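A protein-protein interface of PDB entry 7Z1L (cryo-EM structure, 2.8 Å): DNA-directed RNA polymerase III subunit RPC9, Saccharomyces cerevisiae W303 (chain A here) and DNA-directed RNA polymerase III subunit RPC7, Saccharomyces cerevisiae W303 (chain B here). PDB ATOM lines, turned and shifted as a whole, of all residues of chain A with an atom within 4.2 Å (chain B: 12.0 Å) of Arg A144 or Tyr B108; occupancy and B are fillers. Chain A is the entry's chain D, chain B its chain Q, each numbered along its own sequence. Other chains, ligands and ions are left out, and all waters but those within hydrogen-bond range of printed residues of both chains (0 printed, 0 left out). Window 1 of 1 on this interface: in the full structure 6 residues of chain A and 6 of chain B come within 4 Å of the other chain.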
ATOM      1  N   LYS A 114      13.264 -26.901 -22.173  1.00  0.00           N
ATOM      2  CA  LYS A 114      11.889 -26.639 -21.740  1.00  0.00           C
ATOM      3  C   LYS A 114      11.110 -25.971 -22.874  1.00  0.00           C
ATOM      4  O   LYS A 114      10.686 -24.816 -22.799  1.00  0.00           O
ATOM      5  CB  LYS A 114      11.880 -25.786 -20.477  1.00  0.00           C
ATOM      6  CG  LYS A 114      12.640 -26.389 -19.307  1.00  0.00           C
ATOM      7  CD  LYS A 114      11.752 -27.307 -18.482  1.00  0.00           C
ATOM      8  CE  LYS A 114      12.543 -27.994 -17.380  1.00  0.00           C
ATOM      9  NZ  LYS A 114      13.621 -28.864 -17.925  1.00  0.00           N
ATOM     10  N   PHE A 116       7.960 -26.475 -25.961  1.00  0.00           N
ATOM     11  CA  PHE A 116       6.710 -27.141 -26.287  1.00  0.00           C
ATOM     12  C   PHE A 116       6.754 -27.700 -27.707  1.00  0.00           C
ATOM     13  O   PHE A 116       7.714 -27.501 -28.453  1.00  0.00           O
ATOM     14  CB  PHE A 116       5.534 -26.178 -26.119  1.00  0.00           C
ATOM     15  CG  PHE A 116       5.146 -25.940 -24.688  1.00  0.00           C
ATOM     16  CD1 PHE A 116       5.612 -26.772 -23.682  1.00  0.00           C
ATOM     17  CD2 PHE A 116       4.316 -24.886 -24.347  1.00  0.00           C
ATOM     18  CE1 PHE A 116       5.258 -26.558 -22.365  1.00  0.00           C
ATOM     19  CE2 PHE A 116       3.957 -24.666 -23.030  1.00  0.00           C
ATOM     20  CZ  PHE A 116       4.429 -25.504 -22.039  1.00  0.00           C
ATOM     21  N   GLU A 119       6.639 -24.872 -30.353  1.00  0.00           N
ATOM     22  CA  GLU A 119       7.909 -24.154 -30.361  1.00  0.00           C
ATOM     23  C   GLU A 119       9.008 -24.991 -31.001  1.00  0.00           C
ATOM     24  O   GLU A 119       9.797 -24.487 -31.810  1.00  0.00           O
ATOM     25  CB  GLU A 119       8.292 -23.756 -28.936  1.00  0.00           C
ATOM     26  CG  GLU A 119       7.224 -22.959 -28.207  1.00  0.00           C
ATOM     27  CD  GLU A 119       7.409 -22.975 -26.703  1.00  0.00           C
ATOM     28  OE1 GLU A 119       8.362 -23.626 -26.227  1.00  0.00           O
ATOM     29  OE2 GLU A 119       6.602 -22.338 -25.995  1.00  0.00           O
ATOM     30  N   VAL A 138       9.887 -18.307 -29.567  1.00  0.00           N
ATOM     31  CA  VAL A 138       9.457 -18.828 -28.273  1.00  0.00           C
ATOM     32  C   VAL A 138       9.025 -17.666 -27.387  1.00  0.00           C
ATOM     33  O   VAL A 138       9.687 -16.620 -27.344  1.00  0.00           O
ATOM     34  CB  VAL A 138      10.564 -19.678 -27.617  1.00  0.00           C
ATOM     35  CG1 VAL A 138      11.853 -18.884 -27.427  1.00  0.00           C
ATOM     36  CG2 VAL A 138      10.087 -20.264 -26.293  1.00  0.00           C
ATOM     37  N   GLU A 139       7.889 -17.827 -26.717  1.00  0.00           N
ATOM     38  CA  GLU A 139       7.346 -16.790 -25.853  1.00  0.00           C
ATOM     39  C   GLU A 139       7.905 -16.924 -24.442  1.00  0.00           C
ATOM     40  O   GLU A 139       8.211 -18.027 -23.980  1.00  0.00           O
ATOM     41  CB  GLU A 139       5.819 -16.861 -25.817  1.00  0.00           C
ATOM     42  CG  GLU A 139       5.146 -16.377 -27.089  1.00  0.00           C
ATOM     43  CD  GLU A 139       3.635 -16.452 -27.010  1.00  0.00           C
ATOM     44  OE1 GLU A 139       3.114 -16.789 -25.928  1.00  0.00           O
ATOM     45  OE2 GLU A 139       2.969 -16.176 -28.030  1.00  0.00           O
ATOM     46  N   GLU A 140       8.023 -15.777 -23.763  1.00  0.00           N
ATOM     47  CA  GLU A 140       8.593 -15.687 -22.414  1.00  0.00           C
ATOM     48  C   GLU A 140       9.991 -16.298 -22.364  1.00  0.00           C
ATOM     49  O   GLU A 140      10.336 -17.042 -21.444  1.00  0.00           O
ATOM     50  CB  GLU A 140       7.670 -16.331 -21.376  1.00  0.00           C
ATOM     51  CG  GLU A 140       6.242 -15.805 -21.401  1.00  0.00           C
ATOM     52  CD  GLU A 140       6.125 -14.394 -20.860  1.00  0.00           C
ATOM     53  OE1 GLU A 140       7.000 -13.981 -20.071  1.00  0.00           O
ATOM     54  OE2 GLU A 140       5.155 -13.697 -21.224  1.00  0.00           O
ATOM     55  N   CYS A 141      10.796 -15.980 -23.379  1.00  0.00           N
ATOM     56  CA  CYS A 141      12.130 -16.562 -23.504  1.00  0.00           C
ATOM     57  C   CYS A 141      13.045 -16.120 -22.367  1.00  0.00           C
ATOM     58  O   CYS A 141      13.810 -16.926 -21.824  1.00  0.00           O
ATOM     59  CB  CYS A 141      12.727 -16.178 -24.856  1.00  0.00           C
ATOM     60  SG  CYS A 141      12.735 -14.396 -25.143  1.00  0.00           S
ATOM     61  N   ASP A 142      12.990 -14.838 -22.002  1.00  0.00           N
ATOM     62  CA  ASP A 142      13.876 -14.326 -20.962  1.00  0.00           C
ATOM     63  C   ASP A 142      13.494 -14.869 -19.590  1.00  0.00           C
ATOM     64  O   ASP A 142      14.368 -15.178 -18.772  1.00  0.00           O
ATOM     65  CB  ASP A 142      13.855 -12.798 -20.960  1.00  0.00           C
ATOM     66  CG  ASP A 142      14.298 -12.208 -22.284  1.00  0.00           C
ATOM     67  OD1 ASP A 142      15.101 -12.857 -22.986  1.00  0.00           O
ATOM     68  OD2 ASP A 142      13.843 -11.096 -22.623  1.00  0.00           O
ATOM     69  N   ALA A 143      12.193 -14.985 -19.317  1.00  0.00           N
ATOM     70  CA  ALA A 143      11.755 -15.472 -18.014  1.00  0.00           C
ATOM     71  C   ALA A 143      11.975 -16.974 -17.873  1.00  0.00           C
ATOM     72  O   ALA A 143      12.417 -17.446 -16.819  1.00  0.00           O
ATOM     73  CB  ALA A 143      10.284 -15.122 -17.791  1.00  0.00           C
ATOM     74  N   ARG A 144      11.671 -17.741 -18.923  1.00  0.00           N
ATOM     75  CA  ARG A 144      11.774 -19.194 -18.831  1.00  0.00           C
ATOM     76  C   ARG A 144      13.225 -19.657 -18.859  1.00  0.00           C
ATOM     77  O   ARG A 144      13.608 -20.559 -18.104  1.00  0.00           O
ATOM     78  CB  ARG A 144      10.984 -19.847 -19.966  1.00  0.00           C
ATOM     79  CG  ARG A 144      10.670 -21.317 -19.746  1.00  0.00           C
ATOM     80  CD  ARG A 144      10.130 -21.952 -21.018  1.00  0.00           C
ATOM     81  NE  ARG A 144       9.233 -21.055 -21.738  1.00  0.00           N
ATOM     82  CZ  ARG A 144       8.772 -21.280 -22.961  1.00  0.00           C
ATOM     83  NH1 ARG A 144       9.106 -22.367 -23.637  1.00  0.00           N
ATOM     84  NH2 ARG A 144       7.958 -20.390 -23.521  1.00  0.00           N
ATOM     85  N   PHE A 145      14.045 -19.058 -19.717  1.00  0.00           N
ATOM     86  CA  PHE A 145      15.418 -19.495 -19.931  1.00  0.00           C
ATOM     87  C   PHE A 145      16.386 -18.381 -19.563  1.00  0.00           C
ATOM     88  O   PHE A 145      16.172 -17.221 -19.929  1.00  0.00           O
ATOM     89  CB  PHE A 145      15.642 -19.908 -21.388  1.00  0.00           C
ATOM     90  CG  PHE A 145      14.899 -21.145 -21.796  1.00  0.00           C
ATOM     91  CD1 PHE A 145      15.283 -22.388 -21.319  1.00  0.00           C
ATOM     92  CD2 PHE A 145      13.829 -21.067 -22.671  1.00  0.00           C
ATOM     93  CE1 PHE A 145      14.604 -23.529 -21.700  1.00  0.00           C
ATOM     94  CE2 PHE A 145      13.148 -22.205 -23.056  1.00  0.00           C
ATOM     95  CZ  PHE A 145      13.537 -23.437 -22.570  1.00  0.00           C
ATOM     96  N   ASP B 103      -7.842 -24.786 -29.939  1.00  0.00           N
ATOM     97  CA  ASP B 103      -6.959 -25.601 -30.760  1.00  0.00           C
ATOM     98  C   ASP B 103      -6.166 -26.571 -29.893  1.00  0.00           C
ATOM     99  O   ASP B 103      -5.890 -26.310 -28.718  1.00  0.00           O
ATOM    100  CB  ASP B 103      -6.009 -24.715 -31.565  1.00  0.00           C
ATOM    101  CG  ASP B 103      -6.728 -23.910 -32.628  1.00  0.00           C
ATOM    102  OD1 ASP B 103      -7.767 -24.383 -33.132  1.00  0.00           O
ATOM    103  OD2 ASP B 103      -6.254 -22.803 -32.959  1.00  0.00           O
ATOM    104  N   GLY B 104      -5.793 -27.706 -30.489  1.00  0.00           N
ATOM    105  CA  GLY B 104      -5.091 -28.740 -29.751  1.00  0.00           C
ATOM    106  C   GLY B 104      -3.662 -28.392 -29.393  1.00  0.00           C
ATOM    107  O   GLY B 104      -3.072 -29.054 -28.534  1.00  0.00           O
ATOM    108  N   ILE B 105      -3.090 -27.371 -30.033  1.00  0.00           N
ATOM    109  CA  ILE B 105      -1.714 -26.986 -29.749  1.00  0.00           C
ATOM    110  C   ILE B 105      -1.638 -26.308 -28.389  1.00  0.00           C
ATOM    111  O   ILE B 105      -2.568 -25.609 -27.963  1.00  0.00           O
ATOM    112  CB  ILE B 105      -1.169 -26.076 -30.863  1.00  0.00           C
ATOM    113  CG1 ILE B 105      -2.066 -24.854 -31.054  1.00  0.00           C
ATOM    114  CG2 ILE B 105      -1.058 -26.843 -32.160  1.00  0.00           C
ATOM    115  CD1 ILE B 105      -1.518 -23.856 -32.042  1.00  0.00           C
ATOM    116  N   GLU B 106      -0.529 -26.526 -27.690  1.00  0.00           N
ATOM    117  CA  GLU B 106      -0.309 -25.971 -26.362  1.00  0.00           C
ATOM    118  C   GLU B 106       0.853 -24.990 -26.407  1.00  0.00           C
ATOM    119  O   GLU B 106       1.945 -25.333 -26.872  1.00  0.00           O
ATOM    120  CB  GLU B 106      -0.029 -27.080 -25.346  1.00  0.00           C
ATOM    121  CG  GLU B 106      -1.208 -28.007 -25.101  1.00  0.00           C
ATOM    122  CD  GLU B 106      -2.359 -27.315 -24.397  1.00  0.00           C
ATOM    123  OE1 GLU B 106      -2.099 -26.413 -23.574  1.00  0.00           O
ATOM    124  OE2 GLU B 106      -3.524 -27.672 -24.669  1.00  0.00           O
ATOM    125  N   ARG B 107       0.614 -23.776 -25.926  1.00  0.00           N
ATOM    126  CA  ARG B 107       1.630 -22.737 -25.851  1.00  0.00           C
ATOM    127  C   ARG B 107       1.879 -22.362 -24.396  1.00  0.00           C
ATOM    128  O   ARG B 107       1.161 -22.783 -23.485  1.00  0.00           O
ATOM    129  CB  ARG B 107       1.207 -21.496 -26.646  1.00  0.00           C
ATOM    130  CG  ARG B 107       0.788 -21.770 -28.076  1.00  0.00           C
ATOM    131  CD  ARG B 107       0.523 -20.467 -28.811  1.00  0.00           C
ATOM    132  NE  ARG B 107      -0.384 -20.643 -29.938  1.00  0.00           N
ATOM    133  CZ  ARG B 107      -1.707 -20.666 -29.834  1.00  0.00           C
ATOM    134  NH1 ARG B 107      -2.310 -20.538 -28.664  1.00  0.00           N
ATOM    135  NH2 ARG B 107      -2.441 -20.820 -30.931  1.00  0.00           N
ATOM    136  N   TYR B 108       2.923 -21.558 -24.184  1.00  0.00           N
ATOM    137  CA  TYR B 108       3.162 -21.017 -22.851  1.00  0.00           C
ATOM    138  C   TYR B 108       2.153 -19.930 -22.507  1.00  0.00           C
ATOM    139  O   TYR B 108       1.906 -19.666 -21.326  1.00  0.00           O
ATOM    140  CB  TYR B 108       4.588 -20.478 -22.744  1.00  0.00           C
ATOM    141  CG  TYR B 108       5.120 -20.450 -21.329  1.00  0.00           C
ATOM    142  CD1 TYR B 108       5.212 -21.615 -20.579  1.00  0.00           C
ATOM    143  CD2 TYR B 108       5.529 -19.259 -20.743  1.00  0.00           C
ATOM    144  CE1 TYR B 108       5.696 -21.596 -19.283  1.00  0.00           C
ATOM    145  CE2 TYR B 108       6.015 -19.230 -19.449  1.00  0.00           C
ATOM    146  CZ  TYR B 108       6.097 -20.401 -18.724  1.00  0.00           C
ATOM    147  OH  TYR B 108       6.580 -20.377 -17.436  1.00  0.00           O
ATOM    148  N   SER B 109       1.560 -19.294 -23.522  1.00  0.00           N
ATOM    149  CA  SER B 109       0.511 -18.309 -23.282  1.00  0.00           C
ATOM    150  C   SER B 109      -0.777 -18.947 -22.782  1.00  0.00           C
ATOM    151  O   SER B 109      -1.654 -18.233 -22.283  1.00  0.00           O
ATOM    152  CB  SER B 109       0.233 -17.514 -24.559  1.00  0.00           C
ATOM    153  OG  SER B 109      -0.806 -16.572 -24.356  1.00  0.00           O
ATOM    154  N   ASP B 110      -0.919 -20.268 -22.922  1.00  0.00           N
ATOM    155  CA  ASP B 110      -2.062 -20.954 -22.331  1.00  0.00           C
ATOM    156  C   ASP B 110      -2.008 -20.889 -20.812  1.00  0.00           C
ATOM    157  O   ASP B 110      -3.047 -20.805 -20.146  1.00  0.00           O
ATOM    158  CB  ASP B 110      -2.110 -22.403 -22.813  1.00  0.00           C
ATOM    159  CG  ASP B 110      -2.363 -22.509 -24.303  1.00  0.00           C
ATOM    160  OD1 ASP B 110      -3.142 -21.690 -24.835  1.00  0.00           O
ATOM    161  OD2 ASP B 110      -1.780 -23.407 -24.944  1.00  0.00           O
ATOM    162  N   LYS B 111      -0.806 -20.940 -20.243  1.00  0.00           N
ATOM    163  CA  LYS B 111      -0.634 -20.605 -18.841  1.00  0.00           C
ATOM    164  C   LYS B 111      -0.811 -19.102 -18.645  1.00  0.00           C
ATOM    165  O   LYS B 111      -0.644 -18.307 -19.576  1.00  0.00           O
ATOM    166  CB  LYS B 111       0.742 -21.049 -18.342  1.00  0.00           C
ATOM    167  CG  LYS B 111       0.891 -22.554 -18.198  1.00  0.00           C
ATOM    168  CD  LYS B 111       0.001 -23.090 -17.087  1.00  0.00           C
ATOM    169  CE  LYS B 111       0.195 -24.585 -16.899  1.00  0.00           C
ATOM    170  NZ  LYS B 111      -0.117 -25.345 -18.141  1.00  0.00           N
ATOM    171  N   TYR B 112      -1.156 -18.724 -17.410  1.00  0.00           N
ATOM    172  CA  TYR B 112      -1.518 -17.345 -17.061  1.00  0.00           C
ATOM    173  C   TYR B 112      -2.669 -16.840 -17.929  1.00  0.00           C
ATOM    174  O   TYR B 112      -2.691 -15.686 -18.359  1.00  0.00           O
ATOM    175  CB  TYR B 112      -0.314 -16.401 -17.147  1.00  0.00           C
ATOM    176  CG  TYR B 112       0.731 -16.620 -16.076  1.00  0.00           C
ATOM    177  CD1 TYR B 112       0.432 -17.326 -14.918  1.00  0.00           C
ATOM    178  CD2 TYR B 112       2.018 -16.120 -16.226  1.00  0.00           C
ATOM    179  CE1 TYR B 112       1.386 -17.527 -13.937  1.00  0.00           C
ATOM    180  CE2 TYR B 112       2.978 -16.315 -15.250  1.00  0.00           C
ATOM    181  CZ  TYR B 112       2.657 -17.020 -14.110  1.00  0.00           C
ATOM    182  OH  TYR B 112       3.610 -17.217 -13.137  1.00  0.00           O
ATOM    183  N   LEU B 113      -3.633 -17.719 -18.194  1.00  0.00           N
ATOM    184  CA  LEU B 113      -4.834 -17.379 -18.942  1.00  0.00           C
ATOM    185  C   LEU B 113      -6.052 -17.728 -18.102  1.00  0.00           C
ATOM    186  O   LEU B 113      -6.147 -18.840 -17.571  1.00  0.00           O
ATOM    187  CB  LEU B 113      -4.884 -18.115 -20.284  1.00  0.00           C
ATOM    188  CG  LEU B 113      -6.066 -17.775 -21.194  1.00  0.00           C
ATOM    189  CD1 LEU B 113      -6.157 -16.274 -21.423  1.00  0.00           C
ATOM    190  CD2 LEU B 113      -5.957 -18.516 -22.518  1.00  0.00           C
ATOM    191  N   LYS B 114      -6.973 -16.779 -17.981  1.00  0.00           N
ATOM    192  CA  LYS B 114      -8.146 -16.974 -17.142  1.00  0.00           C
ATOM    193  C   LYS B 114      -9.129 -17.942 -17.789  1.00  0.00           C
ATOM    194  O   LYS B 114      -9.314 -17.945 -19.010  1.00  0.00           O
ATOM    195  CB  LYS B 114      -8.810 -15.623 -16.848  1.00  0.00           C
ATOM    196  CG  LYS B 114      -9.299 -14.833 -18.070  1.00  0.00           C
ATOM    197  CD  LYS B 114     -10.772 -15.070 -18.387  1.00  0.00           C
ATOM    198  CE  LYS B 114     -11.240 -14.190 -19.533  1.00  0.00           C
ATOM    199  NZ  LYS B 114     -12.671 -14.429 -19.867  1.00  0.00           N
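The backbone carbonyl oxygen (O) of Lys A114 lies within hydrogen-bond range of the guanidinium group (NH1) of Arg A144. OE1 of Glu A119 lies within hydrogen-bond range of N of Phe A116, 2.9 Å away. OD2 of Asp B110 is in hydrogen-bond range of N of Arg B107 (2.6 Å). OE1 of Glu A119 lies within salt-bridge range of NH1 of Arg A144 (3.0 Å). O of Glu A139 is in hydrogen-bond range of NH2 of Arg A144, 2.4 Å away.
Phe A116 touches Glu B106. Arg B107 touches Phe A116 (C to CE2, 3.4 Å). Phe A116 touches Tyr B108 (CE2 to N, 3.5 Å). Ser B109 touches Glu A139. Glu A140 touches Tyr B108. Arg A144 touches Tyr B108.
Arg A144 touches one residue of chain B. Tyr B108 touches three residues of chain A. No residue of chain B comes within 4 Å of Val A138. Glu A140 touches one residue of chain B. No residue of chain B comes within 4 Å of Cys A141. Ala A143 touches none of the printed residues of chain B. No residue of chain B comes within 4 Å of Phe A145. Printed residues of chain A within 4 Å of Ser B109: Glu A139. Of the printed residues of chain A, Arg B107 touches Phe A116. Printed residues of chain A within 4 Å of Glu B106: Phe A116 (3.5 Å). The nearest residue of chain B that does not touch Arg A144 is Arg B107 (6.5 Å). The nearest printed residue of chain A that does not touch Tyr B108 is Glu A119 (4.2 Å).
Of the 11 printed residues of chain A, 4 touch a printed residue of chain B.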
